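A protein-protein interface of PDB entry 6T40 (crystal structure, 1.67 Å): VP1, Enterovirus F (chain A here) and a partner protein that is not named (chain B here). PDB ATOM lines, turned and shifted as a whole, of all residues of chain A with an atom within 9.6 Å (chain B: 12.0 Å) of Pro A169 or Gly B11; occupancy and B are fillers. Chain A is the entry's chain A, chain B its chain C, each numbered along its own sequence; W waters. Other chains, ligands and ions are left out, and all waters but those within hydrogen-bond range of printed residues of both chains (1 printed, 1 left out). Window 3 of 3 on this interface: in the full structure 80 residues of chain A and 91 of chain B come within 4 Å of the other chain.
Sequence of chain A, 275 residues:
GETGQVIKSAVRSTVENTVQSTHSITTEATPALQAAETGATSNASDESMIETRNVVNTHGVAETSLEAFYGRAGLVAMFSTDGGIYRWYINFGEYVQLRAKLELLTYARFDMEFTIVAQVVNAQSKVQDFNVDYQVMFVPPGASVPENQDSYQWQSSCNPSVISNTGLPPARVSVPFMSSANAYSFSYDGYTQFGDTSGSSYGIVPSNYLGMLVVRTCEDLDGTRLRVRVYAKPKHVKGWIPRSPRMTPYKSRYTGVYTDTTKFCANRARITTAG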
ATOM      1  N   THR A 115      -4.205 -13.104  27.350  1.00  0.00           N
ATOM      2  CA  THR A 115      -3.186 -13.783  26.564  1.00  0.00           C
ATOM      3  C   THR A 115      -3.823 -15.051  26.016  1.00  0.00           C
ATOM      4  O   THR A 115      -4.473 -15.798  26.751  1.00  0.00           O
ATOM      5  CB  THR A 115      -1.963 -14.136  27.424  1.00  0.00           C
ATOM      6  OG1 THR A 115      -1.440 -12.937  28.014  1.00  0.00           O
ATOM      7  CG2 THR A 115      -0.878 -14.778  26.570  1.00  0.00           C
ATOM      8  N   ILE A 116      -3.644 -15.286  24.723  1.00  0.00           N
ATOM      9  CA  ILE A 116      -4.237 -16.447  24.076  1.00  0.00           C
ATOM     10  C   ILE A 116      -3.183 -17.399  23.521  1.00  0.00           C
ATOM     11  O   ILE A 116      -2.336 -17.006  22.722  1.00  0.00           O
ATOM     12  CB  ILE A 116      -5.181 -15.989  22.942  1.00  0.00           C
ATOM     13  CG1 ILE A 116      -6.280 -15.100  23.535  1.00  0.00           C
ATOM     14  CG2 ILE A 116      -5.784 -17.195  22.227  1.00  0.00           C
ATOM     15  CD1 ILE A 116      -7.193 -14.472  22.510  1.00  0.00           C
ATOM     16  N   VAL A 117      -3.244 -18.651  23.966  1.00  0.00           N
ATOM     17  CA  VAL A 117      -2.313 -19.683  23.525  1.00  0.00           C
ATOM     18  C   VAL A 117      -3.125 -20.716  22.752  1.00  0.00           C
ATOM     19  O   VAL A 117      -4.049 -21.322  23.298  1.00  0.00           O
ATOM     20  CB  VAL A 117      -1.630 -20.374  24.728  1.00  0.00           C
ATOM     21  CG1 VAL A 117      -0.614 -21.396  24.234  1.00  0.00           C
ATOM     22  CG2 VAL A 117      -0.954 -19.330  25.613  1.00  0.00           C
ATOM     23  N   ALA A 118      -2.781 -20.921  21.487  1.00  0.00           N
ATOM     24  CA  ALA A 118      -3.521 -21.864  20.661  1.00  0.00           C
ATOM     25  C   ALA A 118      -2.636 -22.814  19.871  1.00  0.00           C
ATOM     26  O   ALA A 118      -1.517 -22.475  19.489  1.00  0.00           O
ATOM     27  CB  ALA A 118      -4.426 -21.096  19.703  1.00  0.00           C
ATOM     28  N   ASN A 131       1.076 -24.841  11.691  1.00  0.00           N
ATOM     29  CA  ASN A 131       0.846 -23.409  11.840  1.00  0.00           C
ATOM     30  C   ASN A 131      -0.405 -23.008  11.081  1.00  0.00           C
ATOM     31  O   ASN A 131      -0.521 -23.260   9.884  1.00  0.00           O
ATOM     32  CB  ASN A 131       2.037 -22.609  11.308  1.00  0.00           C
ATOM     33  CG  ASN A 131       3.315 -22.894  12.068  1.00  0.00           C
ATOM     34  OD1 ASN A 131       3.283 -23.289  13.233  1.00  0.00           O
ATOM     35  ND2 ASN A 131       4.450 -22.678  11.415  1.00  0.00           N
ATOM     36  N   VAL A 132      -1.345 -22.385  11.780  1.00  0.00           N
ATOM     37  CA  VAL A 132      -2.581 -21.954  11.146  1.00  0.00           C
ATOM     38  C   VAL A 132      -3.001 -20.597  11.694  1.00  0.00           C
ATOM     39  O   VAL A 132      -2.772 -20.296  12.868  1.00  0.00           O
ATOM     40  CB  VAL A 132      -3.720 -22.981  11.387  1.00  0.00           C
ATOM     41  CG1 VAL A 132      -4.059 -23.059  12.872  1.00  0.00           C
ATOM     42  CG2 VAL A 132      -4.951 -22.599  10.574  1.00  0.00           C
ATOM     43  N   TYR A 134      -5.596 -17.925  13.059  1.00  0.00           N
ATOM     44  CA  TYR A 134      -6.853 -17.992  13.786  1.00  0.00           C
ATOM     45  C   TYR A 134      -7.312 -16.576  14.102  1.00  0.00           C
ATOM     46  O   TYR A 134      -6.509 -15.642  14.128  1.00  0.00           O
ATOM     47  CB  TYR A 134      -6.695 -18.817  15.069  1.00  0.00           C
ATOM     48  CG  TYR A 134      -5.741 -18.237  16.091  1.00  0.00           C
ATOM     49  CD1 TYR A 134      -6.177 -17.305  17.031  1.00  0.00           C
ATOM     50  CD2 TYR A 134      -4.400 -18.628  16.122  1.00  0.00           C
ATOM     51  CE1 TYR A 134      -5.305 -16.775  17.981  1.00  0.00           C
ATOM     52  CE2 TYR A 134      -3.516 -18.102  17.068  1.00  0.00           C
ATOM     53  CZ  TYR A 134      -3.978 -17.177  17.994  1.00  0.00           C
ATOM     54  OH  TYR A 134      -3.114 -16.651  18.931  1.00  0.00           O
ATOM     55  N   VAL A 162      -8.598 -10.061  16.865  1.00  0.00           N
ATOM     56  CA  VAL A 162      -7.160 -10.222  16.856  1.00  0.00           C
ATOM     57  C   VAL A 162      -6.917 -11.476  16.029  1.00  0.00           C
ATOM     58  O   VAL A 162      -7.501 -12.533  16.280  1.00  0.00           O
ATOM     59  CB  VAL A 162      -6.545 -10.372  18.272  1.00  0.00           C
ATOM     60  CG1 VAL A 162      -7.087 -11.602  18.969  1.00  0.00           C
ATOM     61  CG2 VAL A 162      -5.026 -10.449  18.155  1.00  0.00           C
ATOM     62  N   ILE A 163      -6.093 -11.329  15.001  1.00  0.00           N
ATOM     63  CA  ILE A 163      -5.755 -12.434  14.124  1.00  0.00           C
ATOM     64  C   ILE A 163      -4.289 -12.764  14.338  1.00  0.00           C
ATOM     65  O   ILE A 163      -3.428 -11.890  14.245  1.00  0.00           O
ATOM     66  CB  ILE A 163      -5.973 -12.053  12.640  1.00  0.00           C
ATOM     67  CG1 ILE A 163      -7.470 -11.902  12.360  1.00  0.00           C
ATOM     68  CG2 ILE A 163      -5.351 -13.106  11.729  1.00  0.00           C
ATOM     69  CD1 ILE A 163      -7.781 -11.364  10.978  1.00  0.00           C
ATOM     70  N   SER A 164      -4.007 -14.018  14.657  1.00  0.00           N
ATOM     71  CA  SER A 164      -2.629 -14.427  14.848  1.00  0.00           C
ATOM     72  C   SER A 164      -2.438 -15.814  14.254  1.00  0.00           C
ATOM     73  O   SER A 164      -3.284 -16.290  13.497  1.00  0.00           O
ATOM     74  CB  SER A 164      -2.250 -14.415  16.330  1.00  0.00           C
ATOM     75  OG  SER A 164      -0.838 -14.482  16.466  1.00  0.00           O
ATOM     76  N   ASN A 165      -1.336 -16.461  14.606  1.00  0.00           N
ATOM     77  CA  ASN A 165      -1.020 -17.774  14.059  1.00  0.00           C
ATOM     78  C   ASN A 165      -0.475 -18.671  15.163  1.00  0.00           C
ATOM     79  O   ASN A 165       0.212 -18.201  16.070  1.00  0.00           O
ATOM     80  CB  ASN A 165       0.018 -17.588  12.942  1.00  0.00           C
ATOM     81  CG  ASN A 165       0.228 -18.835  12.109  1.00  0.00           C
ATOM     82  OD1 ASN A 165       0.775 -19.829  12.582  1.00  0.00           O
ATOM     83  ND2 ASN A 165      -0.205 -18.784  10.853  1.00  0.00           N
ATOM     84  N   THR A 166      -0.785 -19.963  15.096  1.00  0.00           N
ATOM     85  CA  THR A 166      -0.300 -20.894  16.108  1.00  0.00           C
ATOM     86  C   THR A 166       1.223 -20.985  16.039  1.00  0.00           C
ATOM     87  O   THR A 166       1.864 -21.523  16.941  1.00  0.00           O
ATOM     88  CB  THR A 166      -0.908 -22.299  15.919  1.00  0.00           C
ATOM     89  OG1 THR A 166      -0.659 -22.756  14.586  1.00  0.00           O
ATOM     90  CG2 THR A 166      -2.413 -22.264  16.169  1.00  0.00           C
ATOM     91  N   GLY A 167       1.793 -20.446  14.965  1.00  0.00           N
ATOM     92  CA  GLY A 167       3.237 -20.461  14.798  1.00  0.00           C
ATOM     93  C   GLY A 167       3.898 -19.217  15.371  1.00  0.00           C
ATOM     94  O   GLY A 167       5.122 -19.113  15.402  1.00  0.00           O
ATOM     95  N   LEU A 168       3.085 -18.266  15.818  1.00  0.00           N
ATOM     96  CA  LEU A 168       3.594 -17.030  16.409  1.00  0.00           C
ATOM     97  C   LEU A 168       3.459 -17.114  17.923  1.00  0.00           C
ATOM     98  O   LEU A 168       2.835 -18.037  18.444  1.00  0.00           O
ATOM     99  CB  LEU A 168       2.787 -15.828  15.907  1.00  0.00           C
ATOM    100  CG  LEU A 168       3.026 -15.344  14.477  1.00  0.00           C
ATOM    101  CD1 LEU A 168       1.960 -14.319  14.093  1.00  0.00           C
ATOM    102  CD2 LEU A 168       4.422 -14.739  14.376  1.00  0.00           C
ATOM    103  N   PRO A 169       4.058 -16.160  18.655  1.00  0.00           N
ATOM    104  CA  PRO A 169       3.941 -16.195  20.114  1.00  0.00           C
ATOM    105  C   PRO A 169       2.467 -16.010  20.473  1.00  0.00           C
ATOM    106  O   PRO A 169       1.660 -15.620  19.625  1.00  0.00           O
ATOM    107  CB  PRO A 169       4.783 -14.998  20.557  1.00  0.00           C
ATOM    108  CG  PRO A 169       5.830 -14.904  19.482  1.00  0.00           C
ATOM    109  CD  PRO A 169       5.017 -15.125  18.226  1.00  0.00           C
ATOM    110  N   PRO A 170       2.092 -16.292  21.728  1.00  0.00           N
ATOM    111  CA  PRO A 170       0.692 -16.129  22.131  1.00  0.00           C
ATOM    112  C   PRO A 170       0.212 -14.708  21.838  1.00  0.00           C
ATOM    113  O   PRO A 170       0.987 -13.755  21.945  1.00  0.00           O
ATOM    114  CB  PRO A 170       0.732 -16.414  23.630  1.00  0.00           C
ATOM    115  CG  PRO A 170       1.840 -17.426  23.743  1.00  0.00           C
ATOM    116  CD  PRO A 170       2.899 -16.854  22.825  1.00  0.00           C
ATOM    117  N   ALA A 171      -1.053 -14.570  21.455  1.00  0.00           N
ATOM    118  CA  ALA A 171      -1.618 -13.253  21.182  1.00  0.00           C
ATOM    119  C   ALA A 171      -1.863 -12.599  22.537  1.00  0.00           C
ATOM    120  O   ALA A 171      -2.044 -13.291  23.538  1.00  0.00           O
ATOM    121  CB  ALA A 171      -2.929 -13.388  20.420  1.00  0.00           C
ATOM    122  N   ARG A 172      -1.866 -11.271  22.574  1.00  0.00           N
ATOM    123  CA  ARG A 172      -2.083 -10.574  23.835  1.00  0.00           C
ATOM    124  C   ARG A 172      -2.599  -9.156  23.643  1.00  0.00           C
ATOM    125  O   ARG A 172      -2.054  -8.388  22.852  1.00  0.00           O
ATOM    126  CB  ARG A 172      -0.784 -10.534  24.644  1.00  0.00           C
ATOM    127  CG  ARG A 172      -0.868  -9.663  25.890  1.00  0.00           C
ATOM    128  CD  ARG A 172       0.437  -9.691  26.664  1.00  0.00           C
ATOM    129  NE  ARG A 172       0.574 -10.903  27.465  1.00  0.00           N
ATOM    130  CZ  ARG A 172       1.675 -11.229  28.133  1.00  0.00           C
ATOM    131  NH1 ARG A 172       2.739 -10.435  28.087  1.00  0.00           N
ATOM    132  NH2 ARG A 172       1.706 -12.333  28.868  1.00  0.00           N
ATOM    133  N   LEU B   5      19.338  -7.362  18.401  1.00  0.00           N
ATOM    134  CA  LEU B   5      19.688  -8.761  18.584  1.00  0.00           C
ATOM    135  C   LEU B   5      18.694  -9.307  19.600  1.00  0.00           C
ATOM    136  O   LEU B   5      18.747  -8.933  20.771  1.00  0.00           O
ATOM    137  CB  LEU B   5      21.123  -8.878  19.115  1.00  0.00           C
ATOM    138  CG  LEU B   5      21.691 -10.291  19.274  1.00  0.00           C
ATOM    139  CD1 LEU B   5      23.200 -10.262  19.102  1.00  0.00           C
ATOM    140  CD2 LEU B   5      21.309 -10.847  20.632  1.00  0.00           C
ATOM    141  N   TYR B   6      17.770 -10.166  19.173  1.00  0.00           N
ATOM    142  CA  TYR B   6      16.816 -10.676  20.145  1.00  0.00           C
ATOM    143  C   TYR B   6      17.434 -11.797  20.970  1.00  0.00           C
ATOM    144  O   TYR B   6      18.281 -12.562  20.502  1.00  0.00           O
ATOM    145  CB  TYR B   6      15.467 -11.045  19.494  1.00  0.00           C
ATOM    146  CG  TYR B   6      15.433 -12.166  18.488  1.00  0.00           C
ATOM    147  CD1 TYR B   6      15.470 -13.497  18.899  1.00  0.00           C
ATOM    148  CD2 TYR B   6      15.266 -11.898  17.128  1.00  0.00           C
ATOM    149  CE1 TYR B   6      15.328 -14.538  17.980  1.00  0.00           C
ATOM    150  CE2 TYR B   6      15.125 -12.933  16.200  1.00  0.00           C
ATOM    151  CZ  TYR B   6      15.153 -14.249  16.637  1.00  0.00           C
ATOM    152  OH  TYR B   6      14.983 -15.278  15.740  1.00  0.00           O
ATOM    153  N   THR B   7      17.005 -11.866  22.222  1.00  0.00           N
ATOM    154  CA  THR B   7      17.580 -12.781  23.198  1.00  0.00           C
ATOM    155  C   THR B   7      16.712 -13.916  23.725  1.00  0.00           C
ATOM    156  O   THR B   7      15.522 -14.005  23.418  1.00  0.00           O
ATOM    157  CB  THR B   7      18.020 -11.955  24.407  1.00  0.00           C
ATOM    158  OG1 THR B   7      16.859 -11.345  24.991  1.00  0.00           O
ATOM    159  CG2 THR B   7      18.982 -10.846  23.981  1.00  0.00           C
ATOM    160  N   PRO B   8      17.314 -14.813  24.528  1.00  0.00           N
ATOM    161  CA  PRO B   8      16.562 -15.929  25.103  1.00  0.00           C
ATOM    162  C   PRO B   8      15.412 -15.325  25.903  1.00  0.00           C
ATOM    163  O   PRO B   8      15.560 -14.255  26.505  1.00  0.00           O
ATOM    164  CB  PRO B   8      17.592 -16.612  25.996  1.00  0.00           C
ATOM    165  CG  PRO B   8      18.860 -16.430  25.208  1.00  0.00           C
ATOM    166  CD  PRO B   8      18.761 -14.977  24.775  1.00  0.00           C
ATOM    167  N   GLY B   9      14.276 -16.009  25.908  1.00  0.00           N
ATOM    168  CA  GLY B   9      13.111 -15.501  26.605  1.00  0.00           C
ATOM    169  C   GLY B   9      12.145 -14.909  25.592  1.00  0.00           C
ATOM    170  O   GLY B   9      10.952 -14.770  25.862  1.00  0.00           O
ATOM    171  N   SER B  10      12.656 -14.560  24.413  1.00  0.00           N
ATOM    172  CA  SER B  10      11.810 -13.982  23.372  1.00  0.00           C
ATOM    173  C   SER B  10      10.643 -14.898  23.024  1.00  0.00           C
ATOM    174  O   SER B  10      10.825 -16.098  22.811  1.00  0.00           O
ATOM    175  CB  SER B  10      12.626 -13.699  22.103  1.00  0.00           C
ATOM    176  OG  SER B  10      13.522 -12.617  22.299  1.00  0.00           O
ATOM    177  N   GLY B  11       9.447 -14.318  22.981  1.00  0.00           N
ATOM    178  CA  GLY B  11       8.253 -15.070  22.643  1.00  0.00           C
ATOM    179  C   GLY B  11       7.616 -15.833  23.788  1.00  0.00           C
ATOM    180  O   GLY B  11       6.480 -16.298  23.670  1.00  0.00           O
ATOM    181  N   GLN B  12       8.329 -15.964  24.901  1.00  0.00           N
ATOM    182  CA  GLN B  12       7.796 -16.706  26.038  1.00  0.00           C
ATOM    183  C   GLN B  12       6.660 -15.960  26.723  1.00  0.00           C
ATOM    184  O   GLN B  12       6.551 -14.737  26.633  1.00  0.00           O
ATOM    185  CB  GLN B  12       8.897 -16.981  27.065  1.00  0.00           C
ATOM    186  CG  GLN B  12       9.148 -15.817  28.014  1.00  0.00           C
ATOM    187  CD  GLN B  12      10.396 -16.002  28.851  1.00  0.00           C
ATOM    188  OE1 GLN B  12      11.012 -17.069  28.842  1.00  0.00           O
ATOM    189  NE2 GLN B  12      10.776 -14.962  29.584  1.00  0.00           N
ATOM    190  N   PHE B  13       5.821 -16.719  27.416  1.00  0.00           N
ATOM    191  CA  PHE B  13       4.694 -16.172  28.153  1.00  0.00           C
ATOM    192  C   PHE B  13       4.894 -16.500  29.630  1.00  0.00           C
ATOM    193  O   PHE B  13       4.544 -17.585  30.093  1.00  0.00           O
ATOM    194  CB  PHE B  13       3.384 -16.773  27.607  1.00  0.00           C
ATOM    195  CG  PHE B  13       2.172 -16.556  28.488  1.00  0.00           C
ATOM    196  CD1 PHE B  13       2.074 -15.452  29.336  1.00  0.00           C
ATOM    197  CD2 PHE B  13       1.108 -17.456  28.442  1.00  0.00           C
ATOM    198  CE1 PHE B  13       0.936 -15.251  30.125  1.00  0.00           C
ATOM    199  CE2 PHE B  13      -0.034 -17.266  29.226  1.00  0.00           C
ATOM    200  CZ  PHE B  13      -0.120 -16.159  30.070  1.00  0.00           C
ATOM    201  N   LEU B  14       5.511 -15.566  30.352  1.00  0.00           N
ATOM    202  CA  LEU B  14       5.738 -15.706  31.791  1.00  0.00           C
ATOM    203  C   LEU B  14       4.483 -15.096  32.413  1.00  0.00           C
ATOM    204  O   LEU B  14       4.185 -13.926  32.178  1.00  0.00           O
ATOM    205  CB  LEU B  14       6.981 -14.910  32.210  1.00  0.00           C
ATOM    206  CG  LEU B  14       7.226 -14.712  33.711  1.00  0.00           C
ATOM    207  CD1 LEU B  14       7.453 -16.057  34.400  1.00  0.00           C
ATOM    208  CD2 LEU B  14       8.434 -13.801  33.903  1.00  0.00           C
ATOM    209  N   THR B  15       3.744 -15.879  33.196  1.00  0.00           N
ATOM    210  CA  THR B  15       2.498 -15.385  33.776  1.00  0.00           C
ATOM    211  C   THR B  15       2.660 -14.177  34.686  1.00  0.00           C
ATOM    212  O   THR B  15       1.715 -13.416  34.887  1.00  0.00           O
ATOM    213  CB  THR B  15       1.749 -16.493  34.544  1.00  0.00           C
ATOM    214  OG1 THR B  15       2.557 -16.961  35.631  1.00  0.00           O
ATOM    215  CG2 THR B  15       1.426 -17.655  33.608  1.00  0.00           C
ATOM    216  N   ASP B  17       4.896 -11.800  34.039  1.00  0.00           N
ATOM    217  CA  ASP B  17       5.572 -10.737  33.297  1.00  0.00           C
ATOM    218  C   ASP B  17       4.816  -9.428  33.460  1.00  0.00           C
ATOM    219  O   ASP B  17       3.670  -9.410  33.913  1.00  0.00           O
ATOM    220  CB  ASP B  17       5.753 -11.090  31.806  1.00  0.00           C
ATOM    221  CG  ASP B  17       4.438 -11.191  31.039  1.00  0.00           C
ATOM    222  OD1 ASP B  17       3.374 -10.801  31.567  1.00  0.00           O
ATOM    223  OD2 ASP B  17       4.481 -11.659  29.878  1.00  0.00           O
ATOM    224  N   PHE B  19       4.593  -6.247  30.994  1.00  0.00           N
ATOM    225  CA  PHE B  19       4.857  -5.403  29.835  1.00  0.00           C
ATOM    226  C   PHE B  19       3.642  -4.554  29.492  1.00  0.00           C
ATOM    227  O   PHE B  19       2.538  -4.794  29.985  1.00  0.00           O
ATOM    228  CB  PHE B  19       5.188  -6.266  28.612  1.00  0.00           C
ATOM    229  CG  PHE B  19       6.329  -7.220  28.824  1.00  0.00           C
ATOM    230  CD1 PHE B  19       7.596  -6.750  29.151  1.00  0.00           C
ATOM    231  CD2 PHE B  19       6.138  -8.591  28.676  1.00  0.00           C
ATOM    232  CE1 PHE B  19       8.661  -7.632  29.332  1.00  0.00           C
ATOM    233  CE2 PHE B  19       7.196  -9.484  28.853  1.00  0.00           C
ATOM    234  CZ  PHE B  19       8.461  -9.001  29.181  1.00  0.00           C
ATOM    235  N   THR B  21       1.020  -3.321  26.609  1.00  0.00           N
ATOM    236  CA  THR B  21       0.502  -3.951  25.401  1.00  0.00           C
ATOM    237  C   THR B  21      -0.628  -3.127  24.800  1.00  0.00           C
ATOM    238  O   THR B  21      -1.291  -2.364  25.500  1.00  0.00           O
ATOM    239  CB  THR B  21      -0.023  -5.374  25.686  1.00  0.00           C
ATOM    240  OG1 THR B  21      -1.009  -5.322  26.720  1.00  0.00           O
ATOM    241  CG2 THR B  21       1.115  -6.288  26.122  1.00  0.00           C
ATOM    242  N   PRO B  22      -0.858  -3.267  23.486  1.00  0.00           N
ATOM    243  CA  PRO B  22      -1.933  -2.505  22.847  1.00  0.00           C
ATOM    244  C   PRO B  22      -3.283  -2.794  23.489  1.00  0.00           C
ATOM    245  O   PRO B  22      -3.571  -3.927  23.883  1.00  0.00           O
ATOM    246  CB  PRO B  22      -1.862  -2.955  21.385  1.00  0.00           C
ATOM    247  CG  PRO B  22      -1.260  -4.325  21.471  1.00  0.00           C
ATOM    248  CD  PRO B  22      -0.190  -4.151  22.514  1.00  0.00           C
HETATM  249  O   HOH W   1       2.712  -8.276  30.593  1.00  0.00           O
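NH1 of Arg A172 lies within salt-bridge range of OD2 of Asp B17, 2.8 Å away.
NE of Arg A172 lies within hydrogen-bond range of OG1 of Thr A115 (2.9 Å).
Among the printed residues, pairs that only touch across the chains: Arg A172 with Phe B13 (3.2 Å), Arg A172 with Thr B21 (3.5 Å), Pro A170 with Gly B11 (3.7 Å), Thr A115 with Phe B13 (3.7 Å), Pro A169 with Gly B11 (3.8 Å), Arg A172 with Phe B19 (3.9 Å) and Val A117 with Phe B13 (3.97 Å).
Printed residues of chain B within 4 Å of Val A117: Phe B13 (3.97 Å). Asn A131 touches none of the printed residues of chain B. No residue of chain B comes within 4 Å of Leu A168. Of chain B, only Gly B11 (3.8 Å) comes within 4 Å of Pro A169. Of chain B, only Gly B11 (3.7 Å) comes within 4 Å of Pro A170. No residue of chain B comes within 4 Å of Ala A171. Of the printed residues of chain B, Arg A172 touches Phe B13 (3.2 Å), Asp B17 (2.8 Å), Phe B19 (3.9 Å) and Thr B21 (3.5 Å). Pro B8 touches none of the printed residues of chain A. No residue of chain A comes within 4 Å of Ser B10. Of chain A, only Pro A169 and Pro A170 come within 4 Å of Gly B11. Printed residues of chain A within 4 Å of Phe B13: Thr A115, Val A117 and Arg A172. Printed residues of chain A within 4 Å of Thr B21: Arg A172. The nearest residue of chain B that does not touch Pro A169 is Gln B12 (5.7 Å). The nearest printed residue of chain B that does not touch Thr A115 is Asp B17 (6.3 Å).
Of the 15 printed residues of chain B, 5 touch a printed residue of chain A. Printed residues of chain B that touch a printed residue of chain A: Gly B11, Phe B13, Asp B17, Phe B19 and Thr B21. Of the 18 printed residues of chain A, 5 touch a printed residue of chain B. Among the printed residues, 8 pairs touch across the chains.
Water W1 lies within hydrogen-bond range of OD1 of Asp B17 (2.8 Å), N of Phe B19 (2.8 Å) and NH1 of Arg A172 (3.3 Å).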
